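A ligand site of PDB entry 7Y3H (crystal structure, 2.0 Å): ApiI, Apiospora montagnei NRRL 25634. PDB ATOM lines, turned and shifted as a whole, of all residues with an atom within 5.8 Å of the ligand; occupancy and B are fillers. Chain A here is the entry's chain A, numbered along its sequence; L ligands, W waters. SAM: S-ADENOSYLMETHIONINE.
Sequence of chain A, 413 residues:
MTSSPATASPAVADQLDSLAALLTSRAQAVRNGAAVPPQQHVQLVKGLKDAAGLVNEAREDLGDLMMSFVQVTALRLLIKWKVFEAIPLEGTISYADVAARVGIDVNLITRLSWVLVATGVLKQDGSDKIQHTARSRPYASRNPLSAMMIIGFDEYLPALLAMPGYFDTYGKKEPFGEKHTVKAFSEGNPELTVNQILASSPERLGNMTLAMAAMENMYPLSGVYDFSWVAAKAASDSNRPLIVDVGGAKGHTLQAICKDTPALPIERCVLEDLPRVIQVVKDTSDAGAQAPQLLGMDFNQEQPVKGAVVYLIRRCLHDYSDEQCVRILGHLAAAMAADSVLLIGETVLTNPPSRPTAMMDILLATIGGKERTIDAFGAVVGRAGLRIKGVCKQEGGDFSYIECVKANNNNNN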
ATOM      1  N   GLU A 216      -2.293  -4.148 -31.328  1.00  0.00           N
ATOM      2  CA  GLU A 216      -1.998  -4.665 -29.988  1.00  0.00           C
ATOM      3  C   GLU A 216      -1.874  -6.188 -30.002  1.00  0.00           C
ATOM      4  O   GLU A 216      -0.899  -6.746 -29.480  1.00  0.00           O
ATOM      5  CB  GLU A 216      -3.090  -4.224 -29.017  1.00  0.00           C
ATOM      6  CG  GLU A 216      -3.067  -4.918 -27.664  1.00  0.00           C
ATOM      7  CD  GLU A 216      -2.010  -4.369 -26.723  1.00  0.00           C
ATOM      8  OE1 GLU A 216      -2.144  -4.567 -25.494  1.00  0.00           O
ATOM      9  OE2 GLU A 216      -1.039  -3.723 -27.201  1.00  0.00           O
ATOM     10  N   ASP A 245      11.773  -9.055 -21.177  1.00  0.00           N
ATOM     11  CA  ASP A 245      11.135  -8.362 -22.311  1.00  0.00           C
ATOM     12  C   ASP A 245      11.740  -6.963 -22.382  1.00  0.00           C
ATOM     13  O   ASP A 245      11.369  -6.069 -21.625  1.00  0.00           O
ATOM     14  CB  ASP A 245       9.617  -8.332 -22.140  1.00  0.00           C
ATOM     15  CG  ASP A 245       8.866  -7.977 -23.434  1.00  0.00           C
ATOM     16  OD1 ASP A 245       9.497  -7.712 -24.480  1.00  0.00           O
ATOM     17  OD2 ASP A 245       7.624  -7.956 -23.407  1.00  0.00           O
ATOM     18  N   VAL A 246      12.691  -6.791 -23.301  1.00  0.00           N
ATOM     19  CA  VAL A 246      13.470  -5.574 -23.408  1.00  0.00           C
ATOM     20  C   VAL A 246      12.664  -4.558 -24.210  1.00  0.00           C
ATOM     21  O   VAL A 246      12.444  -4.741 -25.412  1.00  0.00           O
ATOM     22  CB  VAL A 246      14.822  -5.836 -24.071  1.00  0.00           C
ATOM     23  CG1 VAL A 246      15.692  -4.588 -24.041  1.00  0.00           C
ATOM     24  CG2 VAL A 246      15.542  -7.018 -23.368  1.00  0.00           C
ATOM     25  N   GLY A 247      12.269  -3.469 -23.562  1.00  0.00           N
ATOM     26  CA  GLY A 247      11.343  -2.518 -24.190  1.00  0.00           C
ATOM     27  C   GLY A 247       9.956  -3.098 -24.402  1.00  0.00           C
ATOM     28  O   GLY A 247       9.354  -2.903 -25.464  1.00  0.00           O
ATOM     29  N   GLY A 248       9.444  -3.826 -23.417  1.00  0.00           N
ATOM     30  CA  GLY A 248       8.203  -4.567 -23.568  1.00  0.00           C
ATOM     31  C   GLY A 248       6.931  -3.799 -23.288  1.00  0.00           C
ATOM     32  O   GLY A 248       5.854  -4.413 -23.315  1.00  0.00           O
ATOM     33  N   ALA A 249       7.022  -2.509 -22.984  1.00  0.00           N
ATOM     34  CA  ALA A 249       5.868  -1.621 -22.841  1.00  0.00           C
ATOM     35  C   ALA A 249       4.998  -2.005 -21.649  1.00  0.00           C
ATOM     36  O   ALA A 249       5.315  -1.663 -20.501  1.00  0.00           O
ATOM     37  CB  ALA A 249       5.018  -1.601 -24.117  1.00  0.00           C
ATOM     38  N   THR A 253       2.808  -9.161 -23.851  1.00  0.00           N
ATOM     39  CA  THR A 253       3.493 -10.307 -24.454  1.00  0.00           C
ATOM     40  C   THR A 253       3.939 -11.290 -23.373  1.00  0.00           C
ATOM     41  O   THR A 253       3.658 -12.491 -23.458  1.00  0.00           O
ATOM     42  CB  THR A 253       4.710  -9.844 -25.250  1.00  0.00           C
ATOM     43  OG1 THR A 253       4.294  -8.896 -26.249  1.00  0.00           O
ATOM     44  CG2 THR A 253       5.390 -11.044 -25.930  1.00  0.00           C
ATOM     45  N   GLU A 272      11.142  -4.794 -18.912  1.00  0.00           N
ATOM     46  CA  GLU A 272      12.047  -3.650 -18.924  1.00  0.00           C
ATOM     47  C   GLU A 272      11.526  -2.610 -19.891  1.00  0.00           C
ATOM     48  O   GLU A 272      11.120  -2.952 -21.011  1.00  0.00           O
ATOM     49  CB  GLU A 272      13.460  -4.075 -19.363  1.00  0.00           C
ATOM     50  CG  GLU A 272      14.172  -4.986 -18.386  1.00  0.00           C
ATOM     51  CD  GLU A 272      15.547  -5.410 -18.885  1.00  0.00           C
ATOM     52  OE1 GLU A 272      15.855  -5.206 -20.089  1.00  0.00           O
ATOM     53  OE2 GLU A 272      16.329  -5.946 -18.067  1.00  0.00           O
ATOM     54  N   ASP A 273      11.532  -1.348 -19.466  1.00  0.00           N
ATOM     55  CA  ASP A 273      11.209  -0.239 -20.365  1.00  0.00           C
ATOM     56  C   ASP A 273      11.741   1.037 -19.728  1.00  0.00           C
ATOM     57  O   ASP A 273      12.401   1.008 -18.682  1.00  0.00           O
ATOM     58  CB  ASP A 273       9.712  -0.173 -20.655  1.00  0.00           C
ATOM     59  CG  ASP A 273       9.417   0.361 -22.027  1.00  0.00           C
ATOM     60  OD1 ASP A 273       9.699   1.557 -22.245  1.00  0.00           O
ATOM     61  OD2 ASP A 273       8.893  -0.392 -22.882  1.00  0.00           O
ATOM     62  N   LEU A 274      11.482   2.173 -20.373  1.00  0.00           N
ATOM     63  CA  LEU A 274      11.901   3.435 -19.798  1.00  0.00           C
ATOM     64  C   LEU A 274      11.229   3.614 -18.430  1.00  0.00           C
ATOM     65  O   LEU A 274      10.115   3.124 -18.205  1.00  0.00           O
ATOM     66  CB  LEU A 274      11.553   4.605 -20.720  1.00  0.00           C
ATOM     67  CG  LEU A 274      12.304   4.691 -22.053  1.00  0.00           C
ATOM     68  CD1 LEU A 274      11.740   5.805 -22.896  1.00  0.00           C
ATOM     69  CD2 LEU A 274      13.796   4.880 -21.820  1.00  0.00           C
ATOM     70  N   VAL A 277       7.687   4.790 -18.469  1.00  0.00           N
ATOM     71  CA  VAL A 277       6.789   3.747 -18.935  1.00  0.00           C
ATOM     72  C   VAL A 277       6.527   2.736 -17.820  1.00  0.00           C
ATOM     73  O   VAL A 277       5.386   2.339 -17.563  1.00  0.00           O
ATOM     74  CB  VAL A 277       7.364   3.057 -20.186  1.00  0.00           C
ATOM     75  CG1 VAL A 277       6.495   1.878 -20.609  1.00  0.00           C
ATOM     76  CG2 VAL A 277       7.477   4.056 -21.336  1.00  0.00           C
ATOM     77  N   MET A 297      14.804   1.250 -17.223  1.00  0.00           N
ATOM     78  CA  MET A 297      16.149   1.146 -17.764  1.00  0.00           C
ATOM     79  C   MET A 297      16.192   1.759 -19.158  1.00  0.00           C
ATOM     80  O   MET A 297      15.158   2.127 -19.731  1.00  0.00           O
ATOM     81  CB  MET A 297      16.647  -0.301 -17.802  1.00  0.00           C
ATOM     82  CG  MET A 297      15.737  -1.305 -18.530  1.00  0.00           C
ATOM     83  SD  MET A 297      15.859  -1.292 -20.349  1.00  0.00           S
ATOM     84  CE  MET A 297      17.437  -2.151 -20.582  1.00  0.00           C
ATOM     85  N   ASP A 298      17.395   1.843 -19.701  1.00  0.00           N
ATOM     86  CA  ASP A 298      17.647   2.388 -21.031  1.00  0.00           C
ATOM     87  C   ASP A 298      18.382   1.300 -21.804  1.00  0.00           C
ATOM     88  O   ASP A 298      19.512   0.940 -21.435  1.00  0.00           O
ATOM     89  CB  ASP A 298      18.471   3.673 -20.898  1.00  0.00           C
ATOM     90  CG  ASP A 298      18.783   4.339 -22.230  1.00  0.00           C
ATOM     91  OD1 ASP A 298      18.593   3.740 -23.307  1.00  0.00           O
ATOM     92  OD2 ASP A 298      19.249   5.503 -22.185  1.00  0.00           O
ATOM     93  N   PHE A 299      17.747   0.743 -22.833  1.00  0.00           N
ATOM     94  CA  PHE A 299      18.404  -0.377 -23.507  1.00  0.00           C
ATOM     95  C   PHE A 299      19.534   0.064 -24.436  1.00  0.00           C
ATOM     96  O   PHE A 299      20.156  -0.778 -25.094  1.00  0.00           O
ATOM     97  CB  PHE A 299      17.381  -1.287 -24.245  1.00  0.00           C
ATOM     98  CG  PHE A 299      16.521  -0.592 -25.311  1.00  0.00           C
ATOM     99  CD1 PHE A 299      17.068   0.157 -26.341  1.00  0.00           C
ATOM    100  CD2 PHE A 299      15.135  -0.796 -25.313  1.00  0.00           C
ATOM    101  CE1 PHE A 299      16.253   0.749 -27.322  1.00  0.00           C
ATOM    102  CE2 PHE A 299      14.304  -0.210 -26.294  1.00  0.00           C
ATOM    103  CZ  PHE A 299      14.867   0.548 -27.287  1.00  0.00           C
ATOM    104  N   ASN A 300      19.853   1.353 -24.474  1.00  0.00           N
ATOM    105  CA  ASN A 300      21.093   1.794 -25.092  1.00  0.00           C
ATOM    106  C   ASN A 300      22.278   1.693 -24.148  1.00  0.00           C
ATOM    107  O   ASN A 300      23.420   1.955 -24.561  1.00  0.00           O
ATOM    108  CB  ASN A 300      20.964   3.231 -25.587  1.00  0.00           C
ATOM    109  CG  ASN A 300      19.882   3.400 -26.630  1.00  0.00           C
ATOM    110  OD1 ASN A 300      20.019   2.933 -27.770  1.00  0.00           O
ATOM    111  ND2 ASN A 300      18.796   4.077 -26.271  1.00  0.00           N
ATOM    112  N   ILE A 313      13.268  -8.721 -27.700  1.00  0.00           N
ATOM    113  CA  ILE A 313      13.237  -7.322 -28.095  1.00  0.00           C
ATOM    114  C   ILE A 313      12.319  -7.209 -29.305  1.00  0.00           C
ATOM    115  O   ILE A 313      12.700  -7.523 -30.432  1.00  0.00           O
ATOM    116  CB  ILE A 313      14.646  -6.734 -28.363  1.00  0.00           C
ATOM    117  CG1 ILE A 313      14.556  -5.220 -28.560  1.00  0.00           C
ATOM    118  CG2 ILE A 313      15.417  -7.426 -29.505  1.00  0.00           C
ATOM    119  CD1 ILE A 313      15.899  -4.517 -28.379  1.00  0.00           C
ATOM    120  N   ARG A 314      11.081  -6.799 -29.051  1.00  0.00           N
ATOM    121  CA  ARG A 314       9.998  -6.865 -30.024  1.00  0.00           C
ATOM    122  C   ARG A 314       9.632  -5.452 -30.457  1.00  0.00           C
ATOM    123  O   ARG A 314       9.287  -4.616 -29.615  1.00  0.00           O
ATOM    124  CB  ARG A 314       8.781  -7.586 -29.429  1.00  0.00           C
ATOM    125  CG  ARG A 314       7.573  -7.712 -30.388  1.00  0.00           C
ATOM    126  CD  ARG A 314       6.405  -8.405 -29.683  1.00  0.00           C
ATOM    127  NE  ARG A 314       5.402  -8.933 -30.596  1.00  0.00           N
ATOM    128  CZ  ARG A 314       4.321  -8.254 -30.982  1.00  0.00           C
ATOM    129  NH1 ARG A 314       4.135  -7.013 -30.538  1.00  0.00           N
ATOM    130  NH2 ARG A 314       3.450  -8.793 -31.828  1.00  0.00           N
ATOM    131  N   ARG A 315       9.682  -5.199 -31.761  1.00  0.00           N
ATOM    132  CA  ARG A 315       9.245  -3.927 -32.348  1.00  0.00           C
ATOM    133  C   ARG A 315       9.992  -2.748 -31.736  1.00  0.00           C
ATOM    134  O   ARG A 315       9.423  -1.660 -31.547  1.00  0.00           O
ATOM    135  CB  ARG A 315       7.725  -3.732 -32.206  1.00  0.00           C
ATOM    136  CG  ARG A 315       6.941  -4.630 -33.142  1.00  0.00           C
ATOM    137  CD  ARG A 315       5.437  -4.654 -32.795  1.00  0.00           C
ATOM    138  NE  ARG A 315       4.857  -3.318 -32.778  1.00  0.00           N
ATOM    139  CZ  ARG A 315       3.576  -3.081 -32.464  1.00  0.00           C
ATOM    140  NH1 ARG A 315       2.771  -4.093 -32.149  1.00  0.00           N
ATOM    141  NH2 ARG A 315       3.112  -1.835 -32.470  1.00  0.00           N
ATOM    142  N   CYS A 316      11.268  -2.940 -31.436  1.00  0.00           N
ATOM    143  CA  CYS A 316      12.129  -1.854 -30.995  1.00  0.00           C
ATOM    144  C   CYS A 316      13.180  -1.480 -32.027  1.00  0.00           C
ATOM    145  O   CYS A 316      13.339  -0.284 -32.322  1.00  0.00           O
ATOM    146  CB  CYS A 316      12.802  -2.205 -29.664  1.00  0.00           C
ATOM    147  SG  CYS A 316      11.606  -2.250 -28.283  1.00  0.00           S
ATOM    148  N   HIS A 318      13.356  -1.492 -35.185  1.00  0.00           N
ATOM    149  CA  HIS A 318      12.994  -0.804 -36.426  1.00  0.00           C
ATOM    150  C   HIS A 318      12.949   0.708 -36.256  1.00  0.00           C
ATOM    151  O   HIS A 318      12.830   1.412 -37.256  1.00  0.00           O
ATOM    152  CB  HIS A 318      11.655  -1.328 -36.980  1.00  0.00           C
ATOM    153  CG  HIS A 318      10.460  -1.013 -36.120  1.00  0.00           C
ATOM    154  ND1 HIS A 318       9.719  -1.994 -35.490  1.00  0.00           N
ATOM    155  CD2 HIS A 318       9.868   0.162 -35.801  1.00  0.00           C
ATOM    156  CE1 HIS A 318       8.724  -1.434 -34.815  1.00  0.00           C
ATOM    157  NE2 HIS A 318       8.792  -0.127 -34.991  1.00  0.00           N
ATOM    158  N   ASP A 319      13.036   1.219 -35.025  1.00  0.00           N
ATOM    159  CA  ASP A 319      13.067   2.664 -34.839  1.00  0.00           C
ATOM    160  C   ASP A 319      14.460   3.270 -35.015  1.00  0.00           C
ATOM    161  O   ASP A 319      14.583   4.499 -34.937  1.00  0.00           O
ATOM    162  CB  ASP A 319      12.507   3.030 -33.458  1.00  0.00           C
ATOM    163  CG  ASP A 319      10.973   3.022 -33.428  1.00  0.00           C
ATOM    164  OD1 ASP A 319      10.350   3.145 -34.499  1.00  0.00           O
ATOM    165  OD2 ASP A 319      10.397   2.897 -32.347  1.00  0.00           O
ATOM    166  N   TYR A 320      15.500   2.476 -35.278  1.00  0.00           N
ATOM    167  CA  TYR A 320      16.879   2.955 -35.121  1.00  0.00           C
ATOM    168  C   TYR A 320      17.767   2.574 -36.300  1.00  0.00           C
ATOM    169  O   TYR A 320      17.491   1.643 -37.060  1.00  0.00           O
ATOM    170  CB  TYR A 320      17.482   2.414 -33.812  1.00  0.00           C
ATOM    171  CG  TYR A 320      16.599   2.699 -32.620  1.00  0.00           C
ATOM    172  CD1 TYR A 320      16.296   4.001 -32.257  1.00  0.00           C
ATOM    173  CD2 TYR A 320      16.044   1.670 -31.899  1.00  0.00           C
ATOM    174  CE1 TYR A 320      15.458   4.270 -31.161  1.00  0.00           C
ATOM    175  CE2 TYR A 320      15.212   1.913 -30.831  1.00  0.00           C
ATOM    176  CZ  TYR A 320      14.921   3.217 -30.459  1.00  0.00           C
ATOM    177  OH  TYR A 320      14.085   3.437 -29.388  1.00  0.00           O
HETATM  178  N   SAM L   1       7.774  -4.510 -27.244  1.00  0.00           N
HETATM  179  CA  SAM L   1       6.439  -3.943 -27.082  1.00  0.00           C
HETATM  180  C   SAM L   1       5.464  -4.535 -28.103  1.00  0.00           C
HETATM  181  O   SAM L   1       4.309  -4.108 -28.216  1.00  0.00           O
HETATM  182  OXT SAM L   1       5.829  -5.448 -28.844  1.00  0.00           O
HETATM  183  CB  SAM L   1       6.457  -2.425 -27.221  1.00  0.00           C
HETATM  184  CG  SAM L   1       7.163  -1.900 -28.466  1.00  0.00           C
HETATM  185  SD  SAM L   1       7.059  -0.076 -28.613  1.00  0.00           S
HETATM  186  CE  SAM L   1       7.081   0.031 -30.409  1.00  0.00           C
HETATM  187  C5' SAM L   1       8.795   0.337 -28.251  1.00  0.00           C
HETATM  188  C4' SAM L   1       9.065   0.318 -26.745  1.00  0.00           C
HETATM  189  O4' SAM L   1      10.432   0.585 -26.484  1.00  0.00           O
HETATM  190  C3' SAM L   1       8.264   1.399 -26.039  1.00  0.00           C
HETATM  191  O3' SAM L   1       7.566   0.816 -24.962  1.00  0.00           O
HETATM  192  C2' SAM L   1       9.299   2.391 -25.526  1.00  0.00           C
HETATM  193  O2' SAM L   1       8.967   2.937 -24.258  1.00  0.00           O
HETATM  194  C1' SAM L   1      10.521   1.502 -25.410  1.00  0.00           C
HETATM  195  N9  SAM L   1      11.805   2.242 -25.449  1.00  0.00           N
HETATM  196  C8  SAM L   1      12.176   3.251 -26.315  1.00  0.00           C
HETATM  197  N7  SAM L   1      13.440   3.624 -26.005  1.00  0.00           N
HETATM  198  C5  SAM L   1      13.861   2.865 -24.952  1.00  0.00           C
HETATM  199  C6  SAM L   1      15.048   2.821 -24.246  1.00  0.00           C
HETATM  200  N6  SAM L   1      16.049   3.641 -24.574  1.00  0.00           N
HETATM  201  N1  SAM L   1      15.188   1.934 -23.198  1.00  0.00           N
HETATM  202  C2  SAM L   1      14.162   1.078 -22.871  1.00  0.00           C
HETATM  203  N3  SAM L   1      12.979   1.108 -23.578  1.00  0.00           N
HETATM  204  C4  SAM L   1      12.832   1.999 -24.605  1.00  0.00           C
HETATM  205  O   HOH W   1      16.108   4.740 -27.533  1.00  0.00           O
HETATM  206  O   HOH W   2       8.436   5.691 -24.581  1.00  0.00           O
HETATM  207  O   HOH W   3      12.183   1.580 -29.332  1.00  0.00           O
HETATM  208  O   HOH W   4       5.409   2.147 -24.372  1.00  0.00           O
HETATM  209  O   HOH W   5       7.618   3.360 -29.064  1.00  0.00           O
HETATM  210  O   HOH W   6      13.594   6.317 -26.448  1.00  0.00           O
HETATM  211  O   HOH W   7      10.304  -6.124 -26.334  1.00  0.00           O
HETATM  212  O   HOH W   8       4.134  -1.009 -29.035  1.00  0.00           O
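The side-chain carboxylate (OD1) of Asp 273 is in hydrogen-bond range of an oxygen (O2') of the ligand, at 2.5 Å. The backbone carbonyl oxygen (O) of Arg 314 lies within hydrogen-bond range of a nitrogen (N) of the ligand. The guanidinium group (NH1) of Arg 314 lies within salt-bridge range of an oxygen (OXT) of the ligand, at 2.9 Å. N6 of the ligand sits at hydrogen-bond distance from OD1 of Asp 298 (2.8 Å). N1 of the ligand sits at hydrogen-bond distance from N of Phe 299. A nitrogen (N) of the ligand lies within hydrogen-bond range of the backbone carbonyl oxygen (O) of Gly 247 (2.9 Å). A nitrogen (N6) of the ligand lies close to the side-chain amide nitrogen of Asn 300, at 3.3 Å. OH of Tyr 320 sits at hydrogen-bond distance from N7 of the ligand. The side-chain sulfur of Cys 316 sits at hydrogen-bond distance from an oxygen (O4') of the ligand (3.6 Å).
The backbone NH (N) of Met 297 lies within hydrogen-bond range of the backbone carbonyl oxygen (O) of Asp 273 (2.8 Å). OD2 of Asp 273 is in hydrogen-bond range of N of Ala 249 (2.8 Å). SG of Cys 316 lies within hydrogen-bond range of O of Arg 314, 3.6 Å away. OD1 of Asp 298 is in hydrogen-bond range of N of Asn 300 (2.9 Å). The side-chain sulfur (SD) of Met 297 lies close to the backbone NH (N) of Phe 299, 3.7 Å away. The side-chain sulfur (SG) of Cys 316 sits at hydrogen-bond distance from the backbone carbonyl oxygen (O) of Gly 247, at 3.7 Å. The backbone carbonyl oxygen of Glu 272 sits at hydrogen-bond distance from the backbone NH of Gly 247. The backbone NH (N) of Gly 248 is in hydrogen-bond range of the backbone carbonyl oxygen (O) of Glu 272 (3.1 Å).
The backbone carbonyl oxygen of Met 297 sits close to a nitrogen (N1) of the ligand, at 3.5 Å. Merely in contact with the ligand: Gly 248 (3.7 Å), Ala 249 (3.5 Å), Leu 274 (3.4 Å), Val 277 (3.5 Å) and Arg 315 (3.1 Å). Hydrophobic or aromatic side chains that line the ligand: Ala 249, Leu 274, Val 277, Met 297 and Phe 299. 14 residues have an atom within 4 Å of the ligand: Gly 247, Gly 248, Ala 249, Asp 273, Leu 274, Val 277, Met 297, Asp 298, Phe 299, Asn 300, Arg 314, Arg 315, Cys 316 and Tyr 320.
Water W1 lies within hydrogen-bond range of OH of Tyr 320 (3.0 Å), ND2 of Asn 300 (3.0 Å) and N6 of the ligand (3.2 Å). Water W3 lies within hydrogen-bond range of OH of Tyr 320 (2.7 Å) and O4' of the ligand (3.5 Å).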
